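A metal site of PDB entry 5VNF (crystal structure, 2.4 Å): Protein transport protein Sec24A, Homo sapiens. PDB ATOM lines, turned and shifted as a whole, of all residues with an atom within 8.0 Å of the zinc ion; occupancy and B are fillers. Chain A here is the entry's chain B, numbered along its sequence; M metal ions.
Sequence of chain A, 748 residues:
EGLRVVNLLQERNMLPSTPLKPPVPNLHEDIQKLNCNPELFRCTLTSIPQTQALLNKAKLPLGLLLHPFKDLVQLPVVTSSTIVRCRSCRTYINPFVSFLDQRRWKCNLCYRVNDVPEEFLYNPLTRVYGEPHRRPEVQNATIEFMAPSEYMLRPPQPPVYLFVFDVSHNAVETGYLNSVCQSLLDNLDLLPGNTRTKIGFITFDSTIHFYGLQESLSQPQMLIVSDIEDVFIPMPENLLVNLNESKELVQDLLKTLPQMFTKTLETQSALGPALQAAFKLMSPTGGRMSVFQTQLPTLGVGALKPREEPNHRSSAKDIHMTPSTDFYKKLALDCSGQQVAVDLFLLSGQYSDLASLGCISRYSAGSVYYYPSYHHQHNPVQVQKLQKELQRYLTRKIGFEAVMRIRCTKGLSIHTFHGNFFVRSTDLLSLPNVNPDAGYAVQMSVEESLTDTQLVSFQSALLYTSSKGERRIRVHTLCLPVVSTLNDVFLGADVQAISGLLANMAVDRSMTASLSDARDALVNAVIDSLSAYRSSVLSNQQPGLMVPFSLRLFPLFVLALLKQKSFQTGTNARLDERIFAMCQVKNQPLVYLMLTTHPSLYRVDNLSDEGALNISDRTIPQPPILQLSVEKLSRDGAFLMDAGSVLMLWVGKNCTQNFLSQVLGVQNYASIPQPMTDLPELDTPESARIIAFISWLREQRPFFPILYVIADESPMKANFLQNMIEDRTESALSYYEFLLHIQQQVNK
O of Cys 89 sits at hydrogen-bond distance from NE of Arg 407.
OG1 of Thr 91 sits close to SG of Cys 89.
ND2 of Asn 114 sits close to SG of Cys 86, 3.5 Å away.
N of Cys 86 sits at hydrogen-bond distance from O of Thr 91, 2.8 Å away.
The side-chain sulfur of Cys 86 sits close to the backbone NH of Ser 88, at 3.3 Å.
SG of Cys 110 lies close to N of Arg 112 (3.7 Å).
The side-chain sulfur (SG) of Cys 107 sits close to the backbone NH (N) of Leu 109 (3.3 Å).
The backbone carbonyl oxygen of Arg 112 sits at hydrogen-bond distance from the backbone NH of Cys 107 (3.0 Å).
SG of Cys 110 is bound to the zinc ion, at 2.1 Å.
The zinc ion is bound by SG of Cys 107.
SG of Cys 86 binds the zinc ion, at 2.3 Å.
SG of Cys 89 is bound to the zinc ion (2.7 Å).
The zinc ion has four donor atoms within binding distance.
The nearest printed residue that does not touch the zinc ion is Thr 91 (4.4 Å).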
ATOM      1  N   ARG A  85      20.213   1.247  31.930  1.00  0.00           N
ATOM      2  CA  ARG A  85      19.165   0.432  31.333  1.00  0.00           C
ATOM      3  C   ARG A  85      19.672  -0.194  30.048  1.00  0.00           C
ATOM      4  O   ARG A  85      20.642   0.272  29.441  1.00  0.00           O
ATOM      5  CB  ARG A  85      17.907   1.263  31.043  1.00  0.00           C
ATOM      6  CG  ARG A  85      17.330   1.949  32.250  1.00  0.00           C
ATOM      7  CD  ARG A  85      16.126   2.795  31.893  1.00  0.00           C
ATOM      8  NE  ARG A  85      14.970   1.980  31.532  1.00  0.00           N
ATOM      9  CZ  ARG A  85      13.762   2.480  31.272  1.00  0.00           C
ATOM     10  NH1 ARG A  85      13.556   3.779  31.345  1.00  0.00           N
ATOM     11  NH2 ARG A  85      12.766   1.665  30.951  1.00  0.00           N
ATOM     12  N   CYS A  86      19.006  -1.271  29.634  1.00  0.00           N
ATOM     13  CA  CYS A  86      19.409  -1.953  28.413  1.00  0.00           C
ATOM     14  C   CYS A  86      19.061  -1.109  27.191  1.00  0.00           C
ATOM     15  O   CYS A  86      17.970  -0.556  27.085  1.00  0.00           O
ATOM     16  CB  CYS A  86      18.713  -3.309  28.328  1.00  0.00           C
ATOM     17  SG  CYS A  86      18.936  -4.083  26.706  1.00  0.00           S
ATOM     18  N   ARG A  87      20.005  -1.041  26.245  1.00  0.00           N
ATOM     19  CA  ARG A  87      19.816  -0.206  25.069  1.00  0.00           C
ATOM     20  C   ARG A  87      18.689  -0.693  24.166  1.00  0.00           C
ATOM     21  O   ARG A  87      18.149   0.115  23.399  1.00  0.00           O
ATOM     22  CB  ARG A  87      21.115  -0.112  24.263  1.00  0.00           C
ATOM     23  CG  ARG A  87      22.105   0.921  24.763  1.00  0.00           C
ATOM     24  CD  ARG A  87      23.348   0.951  23.884  1.00  0.00           C
ATOM     25  NE  ARG A  87      24.234   2.066  24.210  1.00  0.00           N
ATOM     26  CZ  ARG A  87      25.407   2.279  23.624  1.00  0.00           C
ATOM     27  NH1 ARG A  87      25.847   1.461  22.675  1.00  0.00           N
ATOM     28  NH2 ARG A  87      26.148   3.320  23.987  1.00  0.00           N
ATOM     29  N   SER A  88      18.331  -1.976  24.222  1.00  0.00           N
ATOM     30  CA  SER A  88      17.358  -2.548  23.303  1.00  0.00           C
ATOM     31  C   SER A  88      15.950  -2.563  23.882  1.00  0.00           C
ATOM     32  O   SER A  88      15.035  -1.968  23.308  1.00  0.00           O
ATOM     33  CB  SER A  88      17.793  -3.958  22.896  1.00  0.00           C
ATOM     34  OG  SER A  88      18.937  -3.940  22.058  1.00  0.00           O
ATOM     35  N   CYS A  89      15.752  -3.250  25.005  1.00  0.00           N
ATOM     36  CA  CYS A  89      14.417  -3.420  25.588  1.00  0.00           C
ATOM     37  C   CYS A  89      14.205  -2.578  26.838  1.00  0.00           C
ATOM     38  O   CYS A  89      13.204  -2.772  27.526  1.00  0.00           O
ATOM     39  CB  CYS A  89      14.172  -4.896  25.914  1.00  0.00           C
ATOM     40  SG  CYS A  89      15.053  -5.441  27.388  1.00  0.00           S
ATOM     41  N   ARG A  90      15.134  -1.666  27.153  1.00  0.00           N
ATOM     42  CA  ARG A  90      14.998  -0.701  28.245  1.00  0.00           C
ATOM     43  C   ARG A  90      14.841  -1.369  29.614  1.00  0.00           C
ATOM     44  O   ARG A  90      14.266  -0.786  30.533  1.00  0.00           O
ATOM     45  CB  ARG A  90      13.811   0.248  28.005  1.00  0.00           C
ATOM     46  CG  ARG A  90      13.801   0.912  26.631  1.00  0.00           C
ATOM     47  CD  ARG A  90      15.060   1.731  26.387  1.00  0.00           C
ATOM     48  NE  ARG A  90      15.450   2.518  27.553  1.00  0.00           N
ATOM     49  CZ  ARG A  90      14.939   3.705  27.880  1.00  0.00           C
ATOM     50  NH1 ARG A  90      13.988   4.244  27.123  1.00  0.00           N
ATOM     51  NH2 ARG A  90      15.373   4.337  28.955  1.00  0.00           N
ATOM     52  N   THR A  91      15.376  -2.575  29.782  1.00  0.00           N
ATOM     53  CA  THR A  91      15.345  -3.239  31.080  1.00  0.00           C
ATOM     54  C   THR A  91      16.362  -2.612  32.030  1.00  0.00           C
ATOM     55  O   THR A  91      17.525  -2.409  31.666  1.00  0.00           O
ATOM     56  CB  THR A  91      15.635  -4.743  30.916  1.00  0.00           C
ATOM     57  OG1 THR A  91      14.581  -5.353  30.168  1.00  0.00           O
ATOM     58  CG2 THR A  91      15.747  -5.430  32.272  1.00  0.00           C
ATOM     59  N   TYR A  92      15.911  -2.283  33.237  1.00  0.00           N
ATOM     60  CA  TYR A  92      16.804  -1.731  34.250  1.00  0.00           C
ATOM     61  C   TYR A  92      17.820  -2.778  34.696  1.00  0.00           C
ATOM     62  O   TYR A  92      17.453  -3.921  35.001  1.00  0.00           O
ATOM     63  CB  TYR A  92      16.006  -1.233  35.453  1.00  0.00           C
ATOM     64  CG  TYR A  92      14.950  -0.205  35.113  1.00  0.00           C
ATOM     65  CD1 TYR A  92      13.680  -0.585  34.688  1.00  0.00           C
ATOM     66  CD2 TYR A  92      15.217   1.152  35.221  1.00  0.00           C
ATOM     67  CE1 TYR A  92      12.718   0.349  34.367  1.00  0.00           C
ATOM     68  CE2 TYR A  92      14.264   2.096  34.899  1.00  0.00           C
ATOM     69  CZ  TYR A  92      13.014   1.696  34.484  1.00  0.00           C
ATOM     70  OH  TYR A  92      12.070   2.642  34.167  1.00  0.00           O
ATOM     71  N   TRP A 105      27.802  -5.801  30.139  1.00  0.00           N
ATOM     72  CA  TRP A 105      26.821  -6.657  30.801  1.00  0.00           C
ATOM     73  C   TRP A 105      25.794  -7.154  29.793  1.00  0.00           C
ATOM     74  O   TRP A 105      25.345  -6.388  28.923  1.00  0.00           O
ATOM     75  CB  TRP A 105      26.131  -5.918  31.951  1.00  0.00           C
ATOM     76  CG  TRP A 105      25.327  -4.702  31.555  1.00  0.00           C
ATOM     77  CD1 TRP A 105      25.812  -3.446  31.303  1.00  0.00           C
ATOM     78  CD2 TRP A 105      23.908  -4.611  31.415  1.00  0.00           C
ATOM     79  NE1 TRP A 105      24.781  -2.593  31.003  1.00  0.00           N
ATOM     80  CE2 TRP A 105      23.600  -3.281  31.059  1.00  0.00           C
ATOM     81  CE3 TRP A 105      22.858  -5.529  31.540  1.00  0.00           C
ATOM     82  CZ2 TRP A 105      22.288  -2.846  30.843  1.00  0.00           C
ATOM     83  CZ3 TRP A 105      21.555  -5.094  31.328  1.00  0.00           C
ATOM     84  CH2 TRP A 105      21.291  -3.768  30.975  1.00  0.00           C
ATOM     85  N   LYS A 106      25.424  -8.425  29.913  1.00  0.00           N
ATOM     86  CA  LYS A 106      24.467  -9.043  29.019  1.00  0.00           C
ATOM     87  C   LYS A 106      23.084  -9.003  29.644  1.00  0.00           C
ATOM     88  O   LYS A 106      22.867  -9.541  30.745  1.00  0.00           O
ATOM     89  CB  LYS A 106      24.862 -10.483  28.697  1.00  0.00           C
ATOM     90  CG  LYS A 106      23.751 -11.295  28.047  1.00  0.00           C
ATOM     91  CD  LYS A 106      24.227 -12.647  27.565  1.00  0.00           C
ATOM     92  CE  LYS A 106      25.073 -12.512  26.328  1.00  0.00           C
ATOM     93  NZ  LYS A 106      25.570 -13.835  25.866  1.00  0.00           N
ATOM     94  N   CYS A 107      22.144  -8.384  28.937  1.00  0.00           N
ATOM     95  CA  CYS A 107      20.780  -8.214  29.446  1.00  0.00           C
ATOM     96  C   CYS A 107      20.101  -9.575  29.620  1.00  0.00           C
ATOM     97  O   CYS A 107      20.122 -10.413  28.724  1.00  0.00           O
ATOM     98  CB  CYS A 107      19.981  -7.327  28.480  1.00  0.00           C
ATOM     99  SG  CYS A 107      18.190  -7.251  28.742  1.00  0.00           S
ATOM    100  N   ASN A 108      19.491  -9.769  30.783  1.00  0.00           N
ATOM    101  CA  ASN A 108      18.845 -11.041  31.093  1.00  0.00           C
ATOM    102  C   ASN A 108      17.444 -11.161  30.503  1.00  0.00           C
ATOM    103  O   ASN A 108      16.805 -12.213  30.674  1.00  0.00           O
ATOM    104  CB  ASN A 108      18.794 -11.253  32.606  1.00  0.00           C
ATOM    105  CG  ASN A 108      18.173 -10.074  33.328  1.00  0.00           C
ATOM    106  OD1 ASN A 108      18.289  -8.920  32.894  1.00  0.00           O
ATOM    107  ND2 ASN A 108      17.517 -10.351  34.448  1.00  0.00           N
ATOM    108  N   LEU A 109      16.944 -10.142  29.803  1.00  0.00           N
ATOM    109  CA  LEU A 109      15.620 -10.230  29.186  1.00  0.00           C
ATOM    110  C   LEU A 109      15.644 -10.252  27.653  1.00  0.00           C
ATOM    111  O   LEU A 109      14.729 -10.820  27.065  1.00  0.00           O
ATOM    112  CB  LEU A 109      14.727  -9.079  29.675  1.00  0.00           C
ATOM    113  CG  LEU A 109      14.003  -9.377  31.002  1.00  0.00           C
ATOM    114  CD1 LEU A 109      14.960  -9.330  32.195  1.00  0.00           C
ATOM    115  CD2 LEU A 109      12.827  -8.446  31.234  1.00  0.00           C
ATOM    116  N   CYS A 110      16.654  -9.676  27.005  1.00  0.00           N
ATOM    117  CA  CYS A 110      16.764  -9.735  25.557  1.00  0.00           C
ATOM    118  C   CYS A 110      18.151 -10.148  25.063  1.00  0.00           C
ATOM    119  O   CYS A 110      18.381 -10.135  23.850  1.00  0.00           O
ATOM    120  CB  CYS A 110      16.389  -8.379  24.926  1.00  0.00           C
ATOM    121  SG  CYS A 110      17.592  -7.061  25.199  1.00  0.00           S
ATOM    122  N   TYR A 111      19.082 -10.487  25.963  1.00  0.00           N
ATOM    123  CA  TYR A 111      20.395 -11.035  25.650  1.00  0.00           C
ATOM    124  C   TYR A 111      21.295 -10.059  24.895  1.00  0.00           C
ATOM    125  O   TYR A 111      22.385 -10.434  24.466  1.00  0.00           O
ATOM    126  CB  TYR A 111      20.267 -12.354  24.860  1.00  0.00           C
ATOM    127  CG  TYR A 111      19.253 -13.307  25.456  1.00  0.00           C
ATOM    128  CD1 TYR A 111      19.199 -13.545  26.826  1.00  0.00           C
ATOM    129  CD2 TYR A 111      18.326 -13.944  24.642  1.00  0.00           C
ATOM    130  CE1 TYR A 111      18.260 -14.413  27.364  1.00  0.00           C
ATOM    131  CE2 TYR A 111      17.388 -14.812  25.179  1.00  0.00           C
ATOM    132  CZ  TYR A 111      17.362 -15.040  26.534  1.00  0.00           C
ATOM    133  OH  TYR A 111      16.416 -15.910  27.043  1.00  0.00           O
ATOM    134  N   ARG A 112      20.868  -8.800  24.746  1.00  0.00           N
ATOM    135  CA  ARG A 112      21.709  -7.794  24.122  1.00  0.00           C
ATOM    136  C   ARG A 112      22.868  -7.429  25.037  1.00  0.00           C
ATOM    137  O   ARG A 112      22.695  -7.239  26.242  1.00  0.00           O
ATOM    138  CB  ARG A 112      20.891  -6.544  23.789  1.00  0.00           C
ATOM    139  CG  ARG A 112      21.708  -5.290  23.551  1.00  0.00           C
ATOM    140  CD  ARG A 112      22.033  -5.104  22.083  1.00  0.00           C
ATOM    141  NE  ARG A 112      22.914  -3.956  21.853  1.00  0.00           N
ATOM    142  CZ  ARG A 112      22.497  -2.706  21.689  1.00  0.00           C
ATOM    143  NH1 ARG A 112      21.196  -2.422  21.711  1.00  0.00           N
ATOM    144  NH2 ARG A 112      23.372  -1.732  21.494  1.00  0.00           N
ATOM    145  N   VAL A 113      24.069  -7.325  24.468  1.00  0.00           N
ATOM    146  CA  VAL A 113      25.250  -6.924  25.219  1.00  0.00           C
ATOM    147  C   VAL A 113      25.301  -5.402  25.284  1.00  0.00           C
ATOM    148  O   VAL A 113      25.219  -4.723  24.250  1.00  0.00           O
ATOM    149  CB  VAL A 113      26.518  -7.489  24.576  1.00  0.00           C
ATOM    150  CG1 VAL A 113      27.733  -7.172  25.436  1.00  0.00           C
ATOM    151  CG2 VAL A 113      26.374  -8.989  24.353  1.00  0.00           C
ATOM    152  N   ASN A 114      25.456  -4.869  26.490  1.00  0.00           N
ATOM    153  CA  ASN A 114      25.503  -3.432  26.720  1.00  0.00           C
ATOM    154  C   ASN A 114      26.861  -3.039  27.280  1.00  0.00           C
ATOM    155  O   ASN A 114      27.686  -3.885  27.651  1.00  0.00           O
ATOM    156  CB  ASN A 114      24.393  -2.993  27.685  1.00  0.00           C
ATOM    157  CG  ASN A 114      23.018  -3.129  27.093  1.00  0.00           C
ATOM    158  OD1 ASN A 114      22.509  -2.201  26.456  1.00  0.00           O
ATOM    159  ND2 ASN A 114      22.399  -4.290  27.275  1.00  0.00           N
ATOM    160  N   ARG A 407       8.156  -6.225  32.356  1.00  0.00           N
ATOM    161  CA  ARG A 407       8.921  -6.878  31.304  1.00  0.00           C
ATOM    162  C   ARG A 407       9.293  -8.281  31.752  1.00  0.00           C
ATOM    163  O   ARG A 407       9.498  -8.510  32.943  1.00  0.00           O
ATOM    164  CB  ARG A 407      10.175  -6.065  30.982  1.00  0.00           C
ATOM    165  CG  ARG A 407       9.907  -4.646  30.480  1.00  0.00           C
ATOM    166  CD  ARG A 407      11.205  -3.856  30.277  1.00  0.00           C
ATOM    167  NE  ARG A 407      10.990  -2.602  29.579  1.00  0.00           N
ATOM    168  CZ  ARG A 407      11.023  -1.409  30.167  1.00  0.00           C
ATOM    169  NH1 ARG A 407      11.264  -1.304  31.467  1.00  0.00           N
ATOM    170  NH2 ARG A 407      10.829  -0.317  29.446  1.00  0.00           N
HETATM  171 ZN    ZN M   1      17.638  -5.965  27.009  1.00  0.00          ZN
